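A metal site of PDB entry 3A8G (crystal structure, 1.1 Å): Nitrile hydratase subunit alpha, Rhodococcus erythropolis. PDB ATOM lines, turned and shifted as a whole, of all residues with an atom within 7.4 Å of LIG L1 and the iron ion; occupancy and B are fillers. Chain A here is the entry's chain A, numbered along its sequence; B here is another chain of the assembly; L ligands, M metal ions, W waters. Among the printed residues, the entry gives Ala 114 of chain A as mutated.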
ATOM      1  N   GLN A  91     -26.752  -4.649  12.364  1.00  0.00           N
ATOM      2  CA  GLN A  91     -25.598  -5.223  11.637  1.00  0.00           C
ATOM      3  C   GLN A  91     -25.329  -6.665  12.084  1.00  0.00           C
ATOM      4  O   GLN A  91     -24.216  -7.148  12.014  1.00  0.00           O
ATOM      5  CB  GLN A  91     -24.363  -4.338  11.702  1.00  0.00           C
ATOM      6  CG  GLN A  91     -24.597  -2.938  11.105  1.00  0.00           C
ATOM      7  CD  GLN A  91     -24.976  -3.069   9.640  1.00  0.00           C
ATOM      8  OE1 GLN A  91     -24.171  -3.689   8.912  1.00  0.00           O
ATOM      9  NE2 GLN A  91     -26.102  -2.570   9.204  1.00  0.00           N
ATOM     10  N   VAL A 109     -14.069 -10.148   5.343  1.00  0.00           N
ATOM     11  CA  VAL A 109     -13.731  -8.754   5.048  1.00  0.00           C
ATOM     12  C   VAL A 109     -15.013  -8.025   4.588  1.00  0.00           C
ATOM     13  O   VAL A 109     -15.978  -8.690   4.212  1.00  0.00           O
ATOM     14  CB  VAL A 109     -12.635  -8.681   3.980  1.00  0.00           C
ATOM     15  CG1 VAL A 109     -13.145  -9.265   2.613  1.00  0.00           C
ATOM     16  CG2 VAL A 109     -12.067  -7.270   3.768  1.00  0.00           C
ATOM     17  N   CYS A 110     -14.963  -6.710   4.579  1.00  0.00           N
ATOM     18  CA  CYS A 110     -15.906  -5.884   3.801  1.00  0.00           C
ATOM     19  C   CYS A 110     -15.039  -5.019   2.889  1.00  0.00           C
ATOM     20  O   CYS A 110     -14.512  -3.978   3.290  1.00  0.00           O
ATOM     21  CB  CYS A 110     -16.779  -5.022   4.705  1.00  0.00           C
ATOM     22  SG  CYS A 110     -17.880  -3.956   3.762  1.00  0.00           S
ATOM     23  N   SER A 111     -14.810  -5.485   1.652  1.00  0.00           N
ATOM     24  CA  SER A 111     -13.903  -4.733   0.787  1.00  0.00           C
ATOM     25  C   SER A 111     -14.445  -3.370   0.452  1.00  0.00           C
ATOM     26  O   SER A 111     -13.646  -2.450   0.171  1.00  0.00           O
ATOM     27  CB  SER A 111     -13.591  -5.507  -0.475  1.00  0.00           C
ATOM     28  OG  SER A 111     -14.696  -5.586  -1.356  1.00  0.00           O
ATOM     29  N   LEU A 112     -15.770  -3.181   0.460  1.00  0.00           N
ATOM     30  CA  LEU A 112     -16.386  -1.932   0.055  1.00  0.00           C
ATOM     31  C   LEU A 112     -16.493  -0.907   1.186  1.00  0.00           C
ATOM     32  O   LEU A 112     -16.791   0.258   0.871  1.00  0.00           O
ATOM     33  CB  LEU A 112     -17.774  -2.225  -0.564  1.00  0.00           C
ATOM     34  CG  LEU A 112     -17.732  -3.077  -1.848  1.00  0.00           C
ATOM     35  CD1 LEU A 112     -19.149  -3.544  -2.212  1.00  0.00           C
ATOM     36  CD2 LEU A 112     -17.116  -2.271  -3.014  1.00  0.00           C
ATOM     37  N   CSD A 113     -16.297  -1.323   2.448  1.00  0.00           N
ATOM     38  CA  CSD A 113     -16.487  -0.422   3.606  1.00  0.00           C
ATOM     39  CB  CSD A 113     -17.895   0.148   3.701  1.00  0.00           C
ATOM     40  SG  CSD A 113     -19.226  -1.044   3.675  1.00  0.00           S
ATOM     41  C   CSD A 113     -16.024  -1.100   4.916  1.00  0.00           C
ATOM     42  O   CSD A 113     -14.806  -0.985   5.182  1.00  0.00           O
ATOM     43  OD1 CSD A 113     -20.434  -0.252   3.974  1.00  0.00           O
ATOM     44  OD2 CSD A 113     -19.274  -1.607   2.294  1.00  0.00           O
ATOM     45  N   ALA A 114     -16.886  -1.759   5.679  1.00  0.00           N
ATOM     46  CA  ALA A 114     -16.381  -2.240   6.964  1.00  0.00           C
ATOM     47  C   ALA A 114     -17.335  -3.242   7.575  1.00  0.00           C
ATOM     48  O   ALA A 114     -17.164  -3.668   8.763  1.00  0.00           O
ATOM     49  CB  ALA A 114     -16.167  -1.083   7.942  1.00  0.00           C
ATOM     50  N   CSO A 115     -18.345  -3.610   6.804  1.00  0.00           N
ATOM     51  CA  CSO A 115     -19.400  -4.500   7.289  1.00  0.00           C
ATOM     52  CB  CSO A 115     -20.236  -4.969   6.064  1.00  0.00           C
ATOM     53  SG  CSO A 115     -20.692  -3.477   5.117  1.00  0.00           S
ATOM     54  C   CSO A 115     -18.886  -5.717   8.075  1.00  0.00           C
ATOM     55  O   CSO A 115     -17.973  -6.427   7.643  1.00  0.00           O
ATOM     56  OD  CSO A 115     -21.755  -2.786   6.017  1.00  0.00           O
ATOM     57  N   THR A 116     -19.510  -5.886   9.229  1.00  0.00           N
ATOM     58  CA  THR A 116     -19.110  -6.761  10.315  1.00  0.00           C
ATOM     59  C   THR A 116     -20.355  -7.109  11.132  1.00  0.00           C
ATOM     60  O   THR A 116     -21.241  -6.270  11.263  1.00  0.00           O
ATOM     61  CB  THR A 116     -18.164  -5.975  11.233  1.00  0.00           C
ATOM     62  OG1 THR A 116     -16.914  -5.735  10.574  1.00  0.00           O
ATOM     63  CG2 THR A 116     -17.855  -6.669  12.548  1.00  0.00           C
ATOM     64  N   TRP A 118     -21.654  -6.835  14.025  1.00  0.00           N
ATOM     65  CA  TRP A 118     -21.396  -6.003  15.218  1.00  0.00           C
ATOM     66  C   TRP A 118     -21.795  -6.668  16.541  1.00  0.00           C
ATOM     67  O   TRP A 118     -20.985  -6.599  17.481  1.00  0.00           O
ATOM     68  CB  TRP A 118     -22.187  -4.663  15.196  1.00  0.00           C
ATOM     69  CG  TRP A 118     -21.647  -3.679  14.173  1.00  0.00           C
ATOM     70  CD1 TRP A 118     -20.563  -3.757  13.390  1.00  0.00           C
ATOM     71  CD2 TRP A 118     -22.289  -2.433  13.852  1.00  0.00           C
ATOM     72  NE1 TRP A 118     -20.444  -2.624  12.587  1.00  0.00           N
ATOM     73  CE2 TRP A 118     -21.521  -1.801  12.876  1.00  0.00           C
ATOM     74  CE3 TRP A 118     -23.443  -1.841  14.326  1.00  0.00           C
ATOM     75  CZ2 TRP A 118     -21.855  -0.559  12.340  1.00  0.00           C
ATOM     76  CZ3 TRP A 118     -23.798  -0.597  13.816  1.00  0.00           C
ATOM     77  CH2 TRP A 118     -23.018   0.027  12.842  1.00  0.00           C
ATOM     78  N   PRO A 124     -15.924  -3.183  14.131  1.00  0.00           N
ATOM     79  CA  PRO A 124     -14.640  -3.534  13.579  1.00  0.00           C
ATOM     80  C   PRO A 124     -13.551  -2.592  14.069  1.00  0.00           C
ATOM     81  O   PRO A 124     -13.764  -1.395  14.263  1.00  0.00           O
ATOM     82  CB  PRO A 124     -14.824  -3.361  12.073  1.00  0.00           C
ATOM     83  CG  PRO A 124     -15.991  -2.417  11.938  1.00  0.00           C
ATOM     84  CD  PRO A 124     -16.906  -2.746  13.129  1.00  0.00           C
ATOM     85  N   TYR A 128      -9.182  -3.567  10.322  1.00  0.00           N
ATOM     86  CA  TYR A 128     -10.108  -4.295   9.440  1.00  0.00           C
ATOM     87  C   TYR A 128     -10.727  -3.332   8.420  1.00  0.00           C
ATOM     88  O   TYR A 128     -11.082  -3.713   7.303  1.00  0.00           O
ATOM     89  CB  TYR A 128     -11.177  -4.923  10.280  1.00  0.00           C
ATOM     90  CG  TYR A 128     -12.331  -5.615   9.610  1.00  0.00           C
ATOM     91  CD1 TYR A 128     -13.463  -4.974   9.190  1.00  0.00           C
ATOM     92  CD2 TYR A 128     -12.236  -7.021   9.401  1.00  0.00           C
ATOM     93  CE1 TYR A 128     -14.513  -5.618   8.571  1.00  0.00           C
ATOM     94  CE2 TYR A 128     -13.287  -7.670   8.823  1.00  0.00           C
ATOM     95  CZ  TYR A 128     -14.428  -7.001   8.406  1.00  0.00           C
ATOM     96  OH  TYR A 128     -15.493  -7.711   7.875  1.00  0.00           O
ATOM     97  N   LYS A 129     -10.838  -2.046   8.813  1.00  0.00           N
ATOM     98  CA  LYS A 129     -11.352  -0.994   7.977  1.00  0.00           C
ATOM     99  C   LYS A 129     -10.257  -0.390   7.101  1.00  0.00           C
ATOM    100  O   LYS A 129     -10.575   0.465   6.275  1.00  0.00           O
ATOM    101  CB  LYS A 129     -11.949   0.101   8.898  1.00  0.00           C
ATOM    102  CG  LYS A 129     -13.074  -0.504   9.757  1.00  0.00           C
ATOM    103  CD  LYS A 129     -13.754   0.514  10.633  1.00  0.00           C
ATOM    104  CE  LYS A 129     -12.883   1.012  11.722  1.00  0.00           C
ATOM    105  NZ  LYS A 129     -13.674   1.756  12.739  1.00  0.00           N
ATOM    106  N   ARG A 134      -8.692  -4.176   3.129  1.00  0.00           N
ATOM    107  CA  ARG A 134      -9.781  -4.196   2.137  1.00  0.00           C
ATOM    108  C   ARG A 134      -9.248  -4.495   0.731  1.00  0.00           C
ATOM    109  O   ARG A 134      -9.935  -5.183  -0.033  1.00  0.00           O
ATOM    110  CB  ARG A 134     -10.490  -2.836   2.144  1.00  0.00           C
ATOM    111  CG  ARG A 134     -11.319  -2.648   3.414  1.00  0.00           C
ATOM    112  CD  ARG A 134     -11.934  -1.271   3.565  1.00  0.00           C
ATOM    113  NE  ARG A 134     -12.656  -0.886   2.350  1.00  0.00           N
ATOM    114  CZ  ARG A 134     -12.933   0.361   1.975  1.00  0.00           C
ATOM    115  NH1 ARG A 134     -12.656   1.424   2.751  1.00  0.00           N
ATOM    116  NH2 ARG A 134     -13.498   0.543   0.782  1.00  0.00           N
ATOM    117  N   THR A 163     -18.200  -9.243   2.646  1.00  0.00           N
ATOM    118  CA  THR A 163     -19.535  -8.903   3.254  1.00  0.00           C
ATOM    119  C   THR A 163     -20.169  -7.761   2.458  1.00  0.00           C
ATOM    120  O   THR A 163     -20.103  -6.607   2.863  1.00  0.00           O
ATOM    121  CB  THR A 163     -19.302  -8.534   4.715  1.00  0.00           C
ATOM    122  OG1 THR A 163     -18.591  -9.569   5.407  1.00  0.00           O
ATOM    123  CG2 THR A 163     -20.640  -8.353   5.400  1.00  0.00           C
ATOM    124  N   THR A 164     -20.752  -8.120   1.327  1.00  0.00           N
ATOM    125  CA  THR A 164     -21.253  -7.166   0.368  1.00  0.00           C
ATOM    126  C   THR A 164     -22.743  -6.918   0.464  1.00  0.00           C
ATOM    127  O   THR A 164     -23.259  -6.002  -0.227  1.00  0.00           O
ATOM    128  CB  THR A 164     -20.919  -7.657  -1.061  1.00  0.00           C
ATOM    129  OG1 THR A 164     -21.269  -9.046  -1.178  1.00  0.00           O
ATOM    130  CG2 THR A 164     -19.409  -7.558  -1.333  1.00  0.00           C
ATOM    131  N   ARG A 168     -24.228 -11.409   7.694  1.00  0.00           N
ATOM    132  CA  ARG A 168     -23.173 -11.030   8.624  1.00  0.00           C
ATOM    133  C   ARG A 168     -22.544 -12.296   9.126  1.00  0.00           C
ATOM    134  O   ARG A 168     -23.253 -13.211   9.615  1.00  0.00           O
ATOM    135  CB  ARG A 168     -23.713 -10.113   9.727  1.00  0.00           C
ATOM    136  CG  ARG A 168     -24.187  -8.790   9.171  1.00  0.00           C
ATOM    137  CD  ARG A 168     -23.052  -7.838   8.865  1.00  0.00           C
ATOM    138  NE  ARG A 168     -23.514  -6.595   8.251  1.00  0.00           N
ATOM    139  CZ  ARG A 168     -23.852  -6.459   6.956  1.00  0.00           C
ATOM    140  NH1 ARG A 168     -23.737  -7.500   6.136  1.00  0.00           N
ATOM    141  NH2 ARG A 168     -24.298  -5.265   6.539  1.00  0.00           N
ATOM    142  N   TYR B  37     -22.121   7.029  13.893  1.00  0.00           N
ATOM    143  CA  TYR B  37     -23.106   5.931  13.813  1.00  0.00           C
ATOM    144  C   TYR B  37     -24.357   6.268  14.593  1.00  0.00           C
ATOM    145  O   TYR B  37     -25.472   5.932  14.172  1.00  0.00           O
ATOM    146  CB  TYR B  37     -22.508   4.676  14.432  1.00  0.00           C
ATOM    147  CG  TYR B  37     -21.513   3.919  13.583  1.00  0.00           C
ATOM    148  CD1 TYR B  37     -21.228   4.233  12.246  1.00  0.00           C
ATOM    149  CD2 TYR B  37     -20.883   2.833  14.183  1.00  0.00           C
ATOM    150  CE1 TYR B  37     -20.312   3.456  11.578  1.00  0.00           C
ATOM    151  CE2 TYR B  37     -19.950   2.054  13.460  1.00  0.00           C
ATOM    152  CZ  TYR B  37     -19.682   2.391  12.153  1.00  0.00           C
ATOM    153  OH  TYR B  37     -18.769   1.587  11.504  1.00  0.00           O
ATOM    154  N   VAL B  52     -29.849   3.059   5.423  1.00  0.00           N
ATOM    155  CA  VAL B  52     -28.429   2.739   5.600  1.00  0.00           C
ATOM    156  C   VAL B  52     -27.714   2.721   4.240  1.00  0.00           C
ATOM    157  O   VAL B  52     -26.548   3.133   4.098  1.00  0.00           O
ATOM    158  CB  VAL B  52     -28.306   1.377   6.329  1.00  0.00           C
ATOM    159  CG1 VAL B  52     -26.853   0.952   6.382  1.00  0.00           C
ATOM    160  CG2 VAL B  52     -28.821   1.499   7.769  1.00  0.00           C
ATOM    161  N   ARG B  56     -24.081   4.389   2.863  1.00  0.00           N
ATOM    162  CA  ARG B  56     -22.949   3.815   2.116  1.00  0.00           C
ATOM    163  C   ARG B  56     -22.688   4.643   0.856  1.00  0.00           C
ATOM    164  O   ARG B  56     -21.537   4.963   0.535  1.00  0.00           O
ATOM    165  CB  ARG B  56     -23.202   2.363   1.724  1.00  0.00           C
ATOM    166  CG  ARG B  56     -23.372   1.432   2.926  1.00  0.00           C
ATOM    167  CD  ARG B  56     -23.217  -0.021   2.459  1.00  0.00           C
ATOM    168  NE  ARG B  56     -23.282  -0.923   3.601  1.00  0.00           N
ATOM    169  CZ  ARG B  56     -24.424  -1.356   4.133  1.00  0.00           C
ATOM    170  NH1 ARG B  56     -25.593  -1.110   3.543  1.00  0.00           N
ATOM    171  NH2 ARG B  56     -24.398  -2.100   5.218  1.00  0.00           N
ATOM    172  N   TYR B  72     -11.681   6.499   8.704  1.00  0.00           N
ATOM    173  CA  TYR B  72     -13.001   5.892   8.619  1.00  0.00           C
ATOM    174  C   TYR B  72     -14.132   6.661   9.282  1.00  0.00           C
ATOM    175  O   TYR B  72     -15.141   7.027   8.642  1.00  0.00           O
ATOM    176  CB  TYR B  72     -12.889   4.447   9.222  1.00  0.00           C
ATOM    177  CG  TYR B  72     -14.216   3.754   9.111  1.00  0.00           C
ATOM    178  CD1 TYR B  72     -14.559   2.984   7.990  1.00  0.00           C
ATOM    179  CD2 TYR B  72     -15.158   3.782  10.188  1.00  0.00           C
ATOM    180  CE1 TYR B  72     -15.765   2.345   7.913  1.00  0.00           C
ATOM    181  CE2 TYR B  72     -16.376   3.165  10.108  1.00  0.00           C
ATOM    182  CZ  TYR B  72     -16.676   2.422   8.981  1.00  0.00           C
ATOM    183  OH  TYR B  72     -17.886   1.794   8.827  1.00  0.00           O
ATOM    184  N   TYR B  76     -17.870   8.997   7.831  1.00  0.00           N
ATOM    185  CA  TYR B  76     -19.282   8.920   8.188  1.00  0.00           C
ATOM    186  C   TYR B  76     -19.803  10.220   8.791  1.00  0.00           C
ATOM    187  O   TYR B  76     -20.997  10.518   8.598  1.00  0.00           O
ATOM    188  CB  TYR B  76     -19.578   7.691   9.120  1.00  0.00           C
ATOM    189  CG  TYR B  76     -19.328   6.466   8.231  1.00  0.00           C
ATOM    190  CD1 TYR B  76     -20.323   5.879   7.466  1.00  0.00           C
ATOM    191  CD2 TYR B  76     -18.022   6.032   8.096  1.00  0.00           C
ATOM    192  CE1 TYR B  76     -20.002   4.775   6.641  1.00  0.00           C
ATOM    193  CE2 TYR B  76     -17.717   4.991   7.255  1.00  0.00           C
ATOM    194  CZ  TYR B  76     -18.705   4.355   6.511  1.00  0.00           C
ATOM    195  OH  TYR B  76     -18.348   3.334   5.682  1.00  0.00           O
ATOM    196  N   ARG B 141     -23.921  -2.966  -4.909  1.00  0.00           N
ATOM    197  CA  ARG B 141     -23.206  -3.821  -3.955  1.00  0.00           C
ATOM    198  C   ARG B 141     -22.563  -5.002  -4.684  1.00  0.00           C
ATOM    199  O   ARG B 141     -22.571  -6.146  -4.242  1.00  0.00           O
ATOM    200  CB  ARG B 141     -24.127  -4.315  -2.828  1.00  0.00           C
ATOM    201  CG  ARG B 141     -24.594  -3.155  -1.942  1.00  0.00           C
ATOM    202  CD  ARG B 141     -23.420  -2.380  -1.332  1.00  0.00           C
ATOM    203  NE  ARG B 141     -22.672  -3.216  -0.402  1.00  0.00           N
ATOM    204  CZ  ARG B 141     -21.644  -2.738   0.326  1.00  0.00           C
ATOM    205  NH1 ARG B 141     -21.143  -1.531   0.066  1.00  0.00           N
ATOM    206  NH2 ARG B 141     -21.135  -3.523   1.262  1.00  0.00           N
HETATM  207  N1  LIG L   1     -19.501  -1.086   6.530  1.00  0.00           N
HETATM  208  O1  LIG L   1     -20.220  -1.255   7.605  1.00  0.00           O
HETATM  209  C1  LG2 L   2     -21.633   1.618   8.639  1.00  0.00           C
HETATM  210  N1  LG2 L   2     -20.470   1.746   8.655  1.00  0.00           N
HETATM  211  C2  LG2 L   2     -24.019   0.848   8.806  1.00  0.00           C
HETATM  212  C3  LG2 L   2     -22.940   1.506   8.007  1.00  0.00           C
HETATM  213  C4  LG2 L   2     -22.860   0.737   6.702  1.00  0.00           C
HETATM  214  C5  LG2 L   2     -23.463   2.802   7.445  1.00  0.00           C
HETATM  215 FE    FE M   1     -18.748  -2.440   5.271  1.00  0.00          FE
HETATM  216  O   HOH W   1     -19.042  -2.247  10.132  1.00  0.00           O
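Of the 23 residues printed, 4 come within 4 Å of the iron ion.
The nearest printed residue that does not touch the iron ion is Arg 141 of chain B (4.8 Å).
Hydrophobic or aromatic side chains that line LIG L1: Ala 114.
Of the 23 residues printed, 3 come within 4 Å of LIG L1.
The nearest printed residue that does not touch LIG L1 is Tyr 72 of chain B (4.02 Å).
OD of CSO 115 is in hydrogen-bond range of NH2 of Arg 56 of chain B (2.8 Å).
The side-chain hydroxyl of Tyr 128 lies within hydrogen-bond range of O of CSO 115 (2.8 Å).
O of Ala 114 lies within hydrogen-bond range of OG1 of Thr 116 (2.8 Å).
OD1 of CSD 113 lies within salt-bridge range of NE of Arg 56 of chain B.
NH2 of Arg 141 of chain B lies within salt-bridge range of OD2 of CSD 113 (2.9 Å).
SG of Cys 110 sits close to O of Thr 163.
N of Cys 110 sits at hydrogen-bond distance from OH of Tyr 128 (3.5 Å).
OH of Tyr 72 of chain B sits at hydrogen-bond distance from N1 of LG2 L2.
The side-chain hydroxyl (OH) of Tyr 37 of chain B is in hydrogen-bond range of a nitrogen (N1) of LG2 L2 (3.3 Å).
Water W1 lies within hydrogen-bond range of O of Ala 114, NE1 of Trp 118 and O1 of LIG L1.
N of CSO 115 is bound to the iron ion, at 2.0 Å.
The iron ion is bound by a nitrogen (N1) of LIG L1, 2.0 Å away.
The iron ion is bound by N of Ala 114 (2.0 Å).
SG of CSD 113 binds the iron ion (2.2 Å).
The iron ion is bound by SG of CSO 115, 2.2 Å away.
SG of Cys 110 is bound to the iron ion, 2.3 Å away.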
